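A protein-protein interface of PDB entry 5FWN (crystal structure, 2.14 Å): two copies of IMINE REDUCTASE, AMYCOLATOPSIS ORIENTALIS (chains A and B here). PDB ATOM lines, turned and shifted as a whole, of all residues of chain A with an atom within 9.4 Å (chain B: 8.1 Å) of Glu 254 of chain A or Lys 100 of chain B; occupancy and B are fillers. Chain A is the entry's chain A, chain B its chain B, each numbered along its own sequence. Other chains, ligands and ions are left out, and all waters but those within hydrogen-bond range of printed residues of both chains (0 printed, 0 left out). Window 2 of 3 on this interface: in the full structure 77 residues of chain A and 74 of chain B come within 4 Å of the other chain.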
ATOM      1  N   LEU A 191     -26.721  -0.407  29.792  1.00  0.00           N
ATOM      2  CA  LEU A 191     -26.930   0.470  28.685  1.00  0.00           C
ATOM      3  C   LEU A 191     -28.377   0.435  28.214  1.00  0.00           C
ATOM      4  O   LEU A 191     -28.992   1.496  28.049  1.00  0.00           O
ATOM      5  CB  LEU A 191     -25.953   0.156  27.597  1.00  0.00           C
ATOM      6  CG  LEU A 191     -25.869   1.061  26.405  1.00  0.00           C
ATOM      7  CD1 LEU A 191     -25.507   2.475  26.858  1.00  0.00           C
ATOM      8  CD2 LEU A 191     -24.824   0.494  25.471  1.00  0.00           C
ATOM      9  N   SER A 194     -30.800   1.850  30.918  1.00  0.00           N
ATOM     10  CA  SER A 194     -30.856   3.302  31.079  1.00  0.00           C
ATOM     11  C   SER A 194     -31.948   3.920  30.172  1.00  0.00           C
ATOM     12  O   SER A 194     -32.340   5.012  30.414  1.00  0.00           O
ATOM     13  CB  SER A 194     -29.524   3.916  30.751  1.00  0.00           C
ATOM     14  OG  SER A 194     -29.289   3.853  29.369  1.00  0.00           O
ATOM     15  N   ALA A 195     -32.397   3.220  29.126  1.00  0.00           N
ATOM     16  CA  ALA A 195     -33.551   3.652  28.316  1.00  0.00           C
ATOM     17  C   ALA A 195     -34.852   3.102  28.838  1.00  0.00           C
ATOM     18  O   ALA A 195     -35.896   3.333  28.218  1.00  0.00           O
ATOM     19  CB  ALA A 195     -33.412   3.210  26.867  1.00  0.00           C
ATOM     20  N   LYS A 246     -15.761   3.564  19.573  1.00  0.00           N
ATOM     21  CA  LYS A 246     -16.039   5.008  19.754  1.00  0.00           C
ATOM     22  C   LYS A 246     -17.551   5.295  19.796  1.00  0.00           C
ATOM     23  O   LYS A 246     -18.009   6.076  20.612  1.00  0.00           O
ATOM     24  CB  LYS A 246     -15.350   5.863  18.669  1.00  0.00           C
ATOM     25  CG  LYS A 246     -13.818   5.912  18.817  1.00  0.00           C
ATOM     26  CD  LYS A 246     -13.202   6.810  17.762  1.00  0.00           C
ATOM     27  CE  LYS A 246     -11.688   6.764  17.774  1.00  0.00           C
ATOM     28  NZ  LYS A 246     -11.177   7.393  16.516  1.00  0.00           N
ATOM     29  N   HIS A 247     -18.328   4.635  18.926  1.00  0.00           N
ATOM     30  CA  HIS A 247     -19.800   4.738  18.973  1.00  0.00           C
ATOM     31  C   HIS A 247     -20.432   4.168  20.218  1.00  0.00           C
ATOM     32  O   HIS A 247     -21.391   4.741  20.751  1.00  0.00           O
ATOM     33  CB  HIS A 247     -20.448   4.107  17.716  1.00  0.00           C
ATOM     34  CG  HIS A 247     -20.166   4.892  16.483  1.00  0.00           C
ATOM     35  ND1 HIS A 247     -19.961   4.317  15.254  1.00  0.00           N
ATOM     36  CD2 HIS A 247     -19.942   6.214  16.312  1.00  0.00           C
ATOM     37  CE1 HIS A 247     -19.655   5.242  14.369  1.00  0.00           C
ATOM     38  NE2 HIS A 247     -19.642   6.402  14.983  1.00  0.00           N
ATOM     39  N   ILE A 248     -19.899   3.037  20.680  1.00  0.00           N
ATOM     40  CA  ILE A 248     -20.406   2.407  21.909  1.00  0.00           C
ATOM     41  C   ILE A 248     -20.135   3.352  23.090  1.00  0.00           C
ATOM     42  O   ILE A 248     -21.010   3.559  23.891  1.00  0.00           O
ATOM     43  CB  ILE A 248     -19.773   1.041  22.128  1.00  0.00           C
ATOM     44  CG1 ILE A 248     -20.260   0.063  21.038  1.00  0.00           C
ATOM     45  CG2 ILE A 248     -20.103   0.514  23.509  1.00  0.00           C
ATOM     46  CD1 ILE A 248     -19.462  -1.219  20.955  1.00  0.00           C
ATOM     47  N   ILE A 249     -18.927   3.928  23.165  1.00  0.00           N
ATOM     48  CA  ILE A 249     -18.543   4.849  24.224  1.00  0.00           C
ATOM     49  C   ILE A 249     -19.467   6.082  24.114  1.00  0.00           C
ATOM     50  O   ILE A 249     -19.920   6.598  25.114  1.00  0.00           O
ATOM     51  CB  ILE A 249     -17.056   5.275  24.092  1.00  0.00           C
ATOM     52  CG1 ILE A 249     -16.122   4.093  24.356  1.00  0.00           C
ATOM     53  CG2 ILE A 249     -16.724   6.426  25.062  1.00  0.00           C
ATOM     54  CD1 ILE A 249     -14.680   4.304  23.982  1.00  0.00           C
ATOM     55  N   GLY A 250     -19.676   6.566  22.899  1.00  0.00           N
ATOM     56  CA  GLY A 250     -20.510   7.729  22.671  1.00  0.00           C
ATOM     57  C   GLY A 250     -21.929   7.477  23.156  1.00  0.00           C
ATOM     58  O   GLY A 250     -22.501   8.306  23.856  1.00  0.00           O
ATOM     59  N   THR A 251     -22.456   6.302  22.818  1.00  0.00           N
ATOM     60  CA  THR A 251     -23.813   5.945  23.187  1.00  0.00           C
ATOM     61  C   THR A 251     -23.889   5.856  24.711  1.00  0.00           C
ATOM     62  O   THR A 251     -24.855   6.330  25.339  1.00  0.00           O
ATOM     63  CB  THR A 251     -24.180   4.615  22.535  1.00  0.00           C
ATOM     64  OG1 THR A 251     -24.206   4.780  21.117  1.00  0.00           O
ATOM     65  CG2 THR A 251     -25.477   4.095  23.008  1.00  0.00           C
ATOM     66  N   SER A 252     -22.872   5.228  25.298  1.00  0.00           N
ATOM     67  CA  SER A 252     -22.848   5.040  26.746  1.00  0.00           C
ATOM     68  C   SER A 252     -22.852   6.424  27.474  1.00  0.00           C
ATOM     69  O   SER A 252     -23.594   6.617  28.442  1.00  0.00           O
ATOM     70  CB  SER A 252     -21.678   4.100  27.128  1.00  0.00           C
ATOM     71  OG  SER A 252     -21.755   3.683  28.498  1.00  0.00           O
ATOM     72  N   GLN A 253     -22.063   7.372  26.991  1.00  0.00           N
ATOM     73  CA  GLN A 253     -22.083   8.755  27.538  1.00  0.00           C
ATOM     74  C   GLN A 253     -23.440   9.404  27.370  1.00  0.00           C
ATOM     75  O   GLN A 253     -24.017   9.845  28.335  1.00  0.00           O
ATOM     76  CB  GLN A 253     -21.075   9.646  26.827  1.00  0.00           C
ATOM     77  CG  GLN A 253     -19.660   9.261  27.179  1.00  0.00           C
ATOM     78  CD  GLN A 253     -18.585   9.896  26.285  1.00  0.00           C
ATOM     79  OE1 GLN A 253     -18.842  10.293  25.146  1.00  0.00           O
ATOM     80  NE2 GLN A 253     -17.357   9.964  26.808  1.00  0.00           N
ATOM     81  N   GLU A 254     -24.019   9.318  26.181  1.00  0.00           N
ATOM     82  CA  GLU A 254     -25.381   9.859  25.975  1.00  0.00           C
ATOM     83  C   GLU A 254     -26.379   9.313  26.964  1.00  0.00           C
ATOM     84  O   GLU A 254     -27.257  10.014  27.395  1.00  0.00           O
ATOM     85  CB  GLU A 254     -25.961   9.544  24.574  1.00  0.00           C
ATOM     86  CG  GLU A 254     -25.280  10.215  23.414  1.00  0.00           C
ATOM     87  CD  GLU A 254     -25.955   9.934  22.060  1.00  0.00           C
ATOM     88  OE1 GLU A 254     -27.010   9.269  21.999  1.00  0.00           O
ATOM     89  OE2 GLU A 254     -25.382  10.378  21.042  1.00  0.00           O
ATOM     90  N   GLN A 255     -26.261   8.027  27.269  1.00  0.00           N
ATOM     91  CA  GLN A 255     -27.227   7.319  28.130  1.00  0.00           C
ATOM     92  C   GLN A 255     -26.924   7.477  29.614  1.00  0.00           C
ATOM     93  O   GLN A 255     -27.701   6.941  30.427  1.00  0.00           O
ATOM     94  CB  GLN A 255     -27.264   5.811  27.774  1.00  0.00           C
ATOM     95  CG  GLN A 255     -27.793   5.518  26.377  1.00  0.00           C
ATOM     96  CD  GLN A 255     -29.223   6.019  26.151  1.00  0.00           C
ATOM     97  OE1 GLN A 255     -29.494   6.635  25.126  1.00  0.00           O
ATOM     98  NE2 GLN A 255     -30.142   5.728  27.093  1.00  0.00           N
ATOM     99  N   GLY A 256     -25.796   8.135  29.959  1.00  0.00           N
ATOM    100  CA  GLY A 256     -25.359   8.270  31.358  1.00  0.00           C
ATOM    101  C   GLY A 256     -24.858   6.968  32.001  1.00  0.00           C
ATOM    102  O   GLY A 256     -25.068   6.732  33.184  1.00  0.00           O
ATOM    103  N   VAL A 257     -24.261   6.088  31.218  1.00  0.00           N
ATOM    104  CA  VAL A 257     -23.768   4.810  31.770  1.00  0.00           C
ATOM    105  C   VAL A 257     -22.276   4.883  31.759  1.00  0.00           C
ATOM    106  O   VAL A 257     -21.688   5.296  30.761  1.00  0.00           O
ATOM    107  CB  VAL A 257     -24.296   3.641  30.920  1.00  0.00           C
ATOM    108  CG1 VAL A 257     -23.633   2.328  31.335  1.00  0.00           C
ATOM    109  CG2 VAL A 257     -25.803   3.538  31.133  1.00  0.00           C
ATOM    110  N   ASP A 258     -21.665   4.480  32.853  1.00  0.00           N
ATOM    111  CA  ASP A 258     -20.204   4.495  32.990  1.00  0.00           C
ATOM    112  C   ASP A 258     -19.564   3.808  31.753  1.00  0.00           C
ATOM    113  O   ASP A 258     -20.022   2.753  31.284  1.00  0.00           O
ATOM    114  CB  ASP A 258     -19.796   3.765  34.268  1.00  0.00           C
ATOM    115  CG  ASP A 258     -18.347   3.977  34.645  1.00  0.00           C
ATOM    116  OD1 ASP A 258     -17.399   3.915  33.822  1.00  0.00           O
ATOM    117  OD2 ASP A 258     -18.144   4.271  35.803  1.00  0.00           O
ATOM    118  N   THR A 259     -18.548   4.427  31.198  1.00  0.00           N
ATOM    119  CA  THR A 259     -17.920   3.979  29.957  1.00  0.00           C
ATOM    120  C   THR A 259     -16.706   3.063  30.152  1.00  0.00           C
ATOM    121  O   THR A 259     -16.034   2.689  29.196  1.00  0.00           O
ATOM    122  CB  THR A 259     -17.424   5.170  29.145  1.00  0.00           C
ATOM    123  OG1 THR A 259     -16.507   5.932  29.936  1.00  0.00           O
ATOM    124  CG2 THR A 259     -18.588   6.095  28.712  1.00  0.00           C
ATOM    125  N   TYR B  72     -24.770  10.714   9.991  1.00  0.00           N
ATOM    126  CA  TYR B  72     -25.937  11.592   9.763  1.00  0.00           C
ATOM    127  C   TYR B  72     -25.696  12.781   8.821  1.00  0.00           C
ATOM    128  O   TYR B  72     -26.572  13.098   7.998  1.00  0.00           O
ATOM    129  CB  TYR B  72     -26.542  12.097  11.101  1.00  0.00           C
ATOM    130  N   SER B  96     -26.701   4.449  11.736  1.00  0.00           N
ATOM    131  CA  SER B  96     -26.566   5.439  12.859  1.00  0.00           C
ATOM    132  C   SER B  96     -25.466   4.740  13.769  1.00  0.00           C
ATOM    133  O   SER B  96     -25.630   3.568  14.056  1.00  0.00           O
ATOM    134  CB  SER B  96     -27.919   5.702  13.537  1.00  0.00           C
ATOM    135  OG  SER B  96     -28.985   5.990  12.651  1.00  0.00           O
ATOM    136  N   GLY B  97     -24.328   5.277  14.233  1.00  0.00           N
ATOM    137  CA  GLY B  97     -24.100   6.271  15.227  1.00  0.00           C
ATOM    138  C   GLY B  97     -24.395   5.861  16.685  1.00  0.00           C
ATOM    139  O   GLY B  97     -23.829   4.936  17.326  1.00  0.00           O
ATOM    140  N   THR B  98     -25.283   6.665  17.193  1.00  0.00           N
ATOM    141  CA  THR B  98     -25.695   6.681  18.535  1.00  0.00           C
ATOM    142  C   THR B  98     -27.190   6.889  18.434  1.00  0.00           C
ATOM    143  O   THR B  98     -27.664   7.275  17.371  1.00  0.00           O
ATOM    144  CB  THR B  98     -25.093   7.893  19.251  1.00  0.00           C
ATOM    145  OG1 THR B  98     -25.647   9.067  18.675  1.00  0.00           O
ATOM    146  CG2 THR B  98     -23.562   7.990  19.091  1.00  0.00           C
ATOM    147  N   PRO B  99     -27.923   6.719  19.555  1.00  0.00           N
ATOM    148  CA  PRO B  99     -29.346   6.864  19.485  1.00  0.00           C
ATOM    149  C   PRO B  99     -29.779   8.318  19.214  1.00  0.00           C
ATOM    150  O   PRO B  99     -30.783   8.535  18.542  1.00  0.00           O
ATOM    151  CB  PRO B  99     -29.806   6.382  20.867  1.00  0.00           C
ATOM    152  CG  PRO B  99     -28.757   5.415  21.303  1.00  0.00           C
ATOM    153  CD  PRO B  99     -27.514   6.099  20.829  1.00  0.00           C
ATOM    154  N   LYS B 100     -29.034   9.302  19.707  1.00  0.00           N
ATOM    155  CA  LYS B 100     -29.348  10.684  19.378  1.00  0.00           C
ATOM    156  C   LYS B 100     -29.271  10.869  17.849  1.00  0.00           C
ATOM    157  O   LYS B 100     -30.082  11.594  17.285  1.00  0.00           O
ATOM    158  CB  LYS B 100     -28.433  11.672  20.105  1.00  0.00           C
ATOM    159  N   GLU B 101     -28.300  10.242  17.189  1.00  0.00           N
ATOM    160  CA  GLU B 101     -28.227  10.341  15.736  1.00  0.00           C
ATOM    161  C   GLU B 101     -29.433   9.703  15.045  1.00  0.00           C
ATOM    162  O   GLU B 101     -29.988  10.315  14.116  1.00  0.00           O
ATOM    163  CB  GLU B 101     -26.970   9.723  15.177  1.00  0.00           C
ATOM    164  CG  GLU B 101     -25.775  10.611  15.275  1.00  0.00           C
ATOM    165  CD  GLU B 101     -24.536   9.870  14.826  1.00  0.00           C
ATOM    166  OE1 GLU B 101     -24.626   9.024  13.886  1.00  0.00           O
ATOM    167  OE2 GLU B 101     -23.494  10.119  15.458  1.00  0.00           O
ATOM    168  N   ALA B 102     -29.880   8.560  15.547  1.00  0.00           N
ATOM    169  CA  ALA B 102     -31.110   7.945  15.067  1.00  0.00           C
ATOM    170  C   ALA B 102     -32.312   8.884  15.202  1.00  0.00           C
ATOM    171  O   ALA B 102     -33.116   9.040  14.263  1.00  0.00           O
ATOM    172  CB  ALA B 102     -31.366   6.626  15.770  1.00  0.00           C
ATOM    173  N   ASN B 103     -32.431   9.528  16.345  1.00  0.00           N
ATOM    174  CA  ASN B 103     -33.550  10.467  16.567  1.00  0.00           C
ATOM    175  C   ASN B 103     -33.451  11.719  15.678  1.00  0.00           C
ATOM    176  O   ASN B 103     -34.453  12.198  15.200  1.00  0.00           O
ATOM    177  CB  ASN B 103     -33.614  10.974  18.014  1.00  0.00           C
ATOM    178  CG  ASN B 103     -33.841   9.888  19.051  1.00  0.00           C
ATOM    179  OD1 ASN B 103     -33.494  10.079  20.232  1.00  0.00           O
ATOM    180  ND2 ASN B 103     -34.381   8.775  18.662  1.00  0.00           N
ATOM    181  N   GLU B 104     -32.255  12.215  15.454  1.00  0.00           N
ATOM    182  CA  GLU B 104     -32.027  13.305  14.518  1.00  0.00           C
ATOM    183  C   GLU B 104     -32.490  12.905  13.110  1.00  0.00           C
ATOM    184  O   GLU B 104     -33.097  13.719  12.415  1.00  0.00           O
ATOM    185  CB  GLU B 104     -30.543  13.657  14.379  1.00  0.00           C
ATOM    186  CG  GLU B 104     -29.975  14.839  15.132  1.00  0.00           C
ATOM    187  CD  GLU B 104     -28.671  15.255  14.452  1.00  0.00           C
ATOM    188  OE1 GLU B 104     -27.707  14.498  14.647  1.00  0.00           O
ATOM    189  OE2 GLU B 104     -28.628  16.237  13.658  1.00  0.00           O
ATOM    190  N   ALA B 105     -32.167  11.679  12.684  1.00  0.00           N
ATOM    191  CA  ALA B 105     -32.593  11.240  11.346  1.00  0.00           C
ATOM    192  C   ALA B 105     -34.099  11.053  11.267  1.00  0.00           C
ATOM    193  O   ALA B 105     -34.717  11.375  10.227  1.00  0.00           O
ATOM    194  CB  ALA B 105     -31.877   9.965  10.895  1.00  0.00           C
ATOM    195  N   LEU B 106     -34.720  10.523  12.324  1.00  0.00           N
ATOM    196  CA  LEU B 106     -36.188  10.444  12.321  1.00  0.00           C
ATOM    197  C   LEU B 106     -36.782  11.834  12.073  1.00  0.00           C
ATOM    198  O   LEU B 106     -37.736  11.994  11.315  1.00  0.00           O
ATOM    199  CB  LEU B 106     -36.712   9.895  13.635  1.00  0.00           C
ATOM    200  CG  LEU B 106     -38.224   9.995  13.852  1.00  0.00           C
ATOM    201  CD1 LEU B 106     -38.957   9.071  12.898  1.00  0.00           C
ATOM    202  CD2 LEU B 106     -38.593   9.717  15.304  1.00  0.00           C
ATOM    203  N   ARG B 107     -36.226  12.835  12.745  1.00  0.00           N
ATOM    204  CA  ARG B 107     -36.768  14.200  12.644  1.00  0.00           C
ATOM    205  C   ARG B 107     -36.644  14.714  11.224  1.00  0.00           C
ATOM    206  O   ARG B 107     -37.569  15.327  10.681  1.00  0.00           O
ATOM    207  CB  ARG B 107     -36.007  15.151  13.550  1.00  0.00           C
ATOM    208  CG  ARG B 107     -36.517  15.349  14.958  1.00  0.00           C
ATOM    209  CD  ARG B 107     -35.432  15.788  15.973  1.00  0.00           C
ATOM    210  NE  ARG B 107     -34.873  17.115  15.621  1.00  0.00           N
ATOM    211  CZ  ARG B 107     -33.589  17.527  15.717  1.00  0.00           C
ATOM    212  NH1 ARG B 107     -32.611  16.732  16.140  1.00  0.00           N
ATOM    213  NH2 ARG B 107     -33.270  18.775  15.357  1.00  0.00           N
ATOM    214  N   ALA B 164     -37.029   5.509  17.497  1.00  0.00           N
ATOM    215  CA  ALA B 164     -35.994   5.494  16.486  1.00  0.00           C
ATOM    216  C   ALA B 164     -34.675   4.938  16.981  1.00  0.00           C
ATOM    217  O   ALA B 164     -34.004   4.243  16.250  1.00  0.00           O
ATOM    218  CB  ALA B 164     -35.792   6.907  15.911  1.00  0.00           C
ATOM    219  N   GLY B 165     -34.297   5.259  18.221  1.00  0.00           N
ATOM    220  CA  GLY B 165     -32.980   4.903  18.756  1.00  0.00           C
ATOM    221  C   GLY B 165     -32.733   3.486  19.291  1.00  0.00           C
ATOM    222  O   GLY B 165     -31.619   3.168  19.693  1.00  0.00           O
ATOM    223  N   VAL B 168     -29.938   1.048  17.563  1.00  0.00           N
ATOM    224  CA  VAL B 168     -28.580   1.446  17.897  1.00  0.00           C
ATOM    225  C   VAL B 168     -28.262   1.147  19.355  1.00  0.00           C
ATOM    226  O   VAL B 168     -27.145   0.739  19.701  1.00  0.00           O
ATOM    227  CB  VAL B 168     -28.340   2.943  17.644  1.00  0.00           C
ATOM    228  CG1 VAL B 168     -26.976   3.363  18.185  1.00  0.00           C
ATOM    229  CG2 VAL B 168     -28.325   3.189  16.178  1.00  0.00           C
ATOM    230  N   LEU B 169     -29.242   1.348  20.215  1.00  0.00           N
ATOM    231  CA  LEU B 169     -29.040   1.055  21.623  1.00  0.00           C
ATOM    232  C   LEU B 169     -28.754  -0.441  21.827  1.00  0.00           C
ATOM    233  O   LEU B 169     -27.788  -0.792  22.459  1.00  0.00           O
ATOM    234  CB  LEU B 169     -30.253   1.473  22.420  1.00  0.00           C
ATOM    235  CG  LEU B 169     -30.094   1.347  23.933  1.00  0.00           C
ATOM    236  CD1 LEU B 169     -29.138   2.431  24.427  1.00  0.00           C
ATOM    237  CD2 LEU B 169     -31.423   1.499  24.609  1.00  0.00           C
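The side-chain carboxylate (OE1) of Glu 254 of chain A sits at hydrogen-bond distance from the backbone NH (N) of Lys 100 of chain B (3.1 Å). The side-chain carboxylate (OE2) of Glu 254 of chain A sits at hydrogen-bond distance from the side-chain hydroxyl (OG1) of Thr 98 of chain B (2.7 Å).
O of Leu 191 of chain A lies within hydrogen-bond range of OG of Ser 194 of chain A (2.7 Å). The side-chain hydroxyl of Thr 98 of chain B lies within hydrogen-bond range of the backbone NH of Glu 101 of chain B, 3.3 Å away. The side-chain hydroxyl (OG) of Ser 194 of chain A lies within hydrogen-bond range of the side-chain amide nitrogen (NE2) of Gln 255 of chain A. The backbone carbonyl oxygen (O) of His 247 of chain A sits at hydrogen-bond distance from the side-chain hydroxyl (OG1) of Thr 251 of chain A (2.8 Å).
Among the printed residues, merely in contact across the chains: Leu 191 of chain A with Leu 169 of chain B, Ala 195 of chain A with Leu 169 of chain B, His 247 of chain A with Gly 97 of chain B, Thr 251 of chain A with Gly 97 of chain B, Thr 251 of chain A with Thr 98 of chain B, Thr 251 of chain A with Pro 99 of chain B, Glu 254 of chain A with Pro 99 of chain B and Gln 255 of chain A with Leu 169 of chain B.
Glu 254 of chain A touches just these residues of chain B: Thr 98 (2.7 Å), Pro 99 (3.4 Å) and Lys 100 (3.1 Å). Lys 100 of chain B touches just one residue of chain A: Glu 254 (3.1 Å). Of chain A, only Thr 251 (3.5 Å) and Glu 254 (2.7 Å) come within 4 Å of Thr 98 of chain B. Pro 99 of chain B touches just these residues of chain A: Thr 251 and Glu 254. Asn 103 of chain B touches none of the printed residues of chain A. Printed residues of chain A within 4 Å of Leu 169 of chain B: Leu 191 (3.7 Å), Ala 195 (3.5 Å) and Gln 255 (3.9 Å). Printed residues of chain A within 4 Å of Gly 97 of chain B: His 247 (3.5 Å) and Thr 251 (3.8 Å). Of the printed residues of chain B, Thr 251 of chain A touches Gly 97 (3.8 Å), Thr 98 (3.5 Å) and Pro 99 (3.6 Å). Ala 105 of chain B touches none of the printed residues of chain A. Val 168 of chain B touches none of the printed residues of chain A.
Of the 17 printed residues of chain A, 6 touch a printed residue of chain B. Printed residues of chain A that touch a printed residue of chain B: Leu 191, Ala 195, His 247, Thr 251, Glu 254 and Gln 255. Among the printed residues, 10 pairs touch across the chains.
No position is printed for both chains. Of the 10 pairs that touch across the chains among the printed residues, none has its exchanged pair printed and touching as well.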
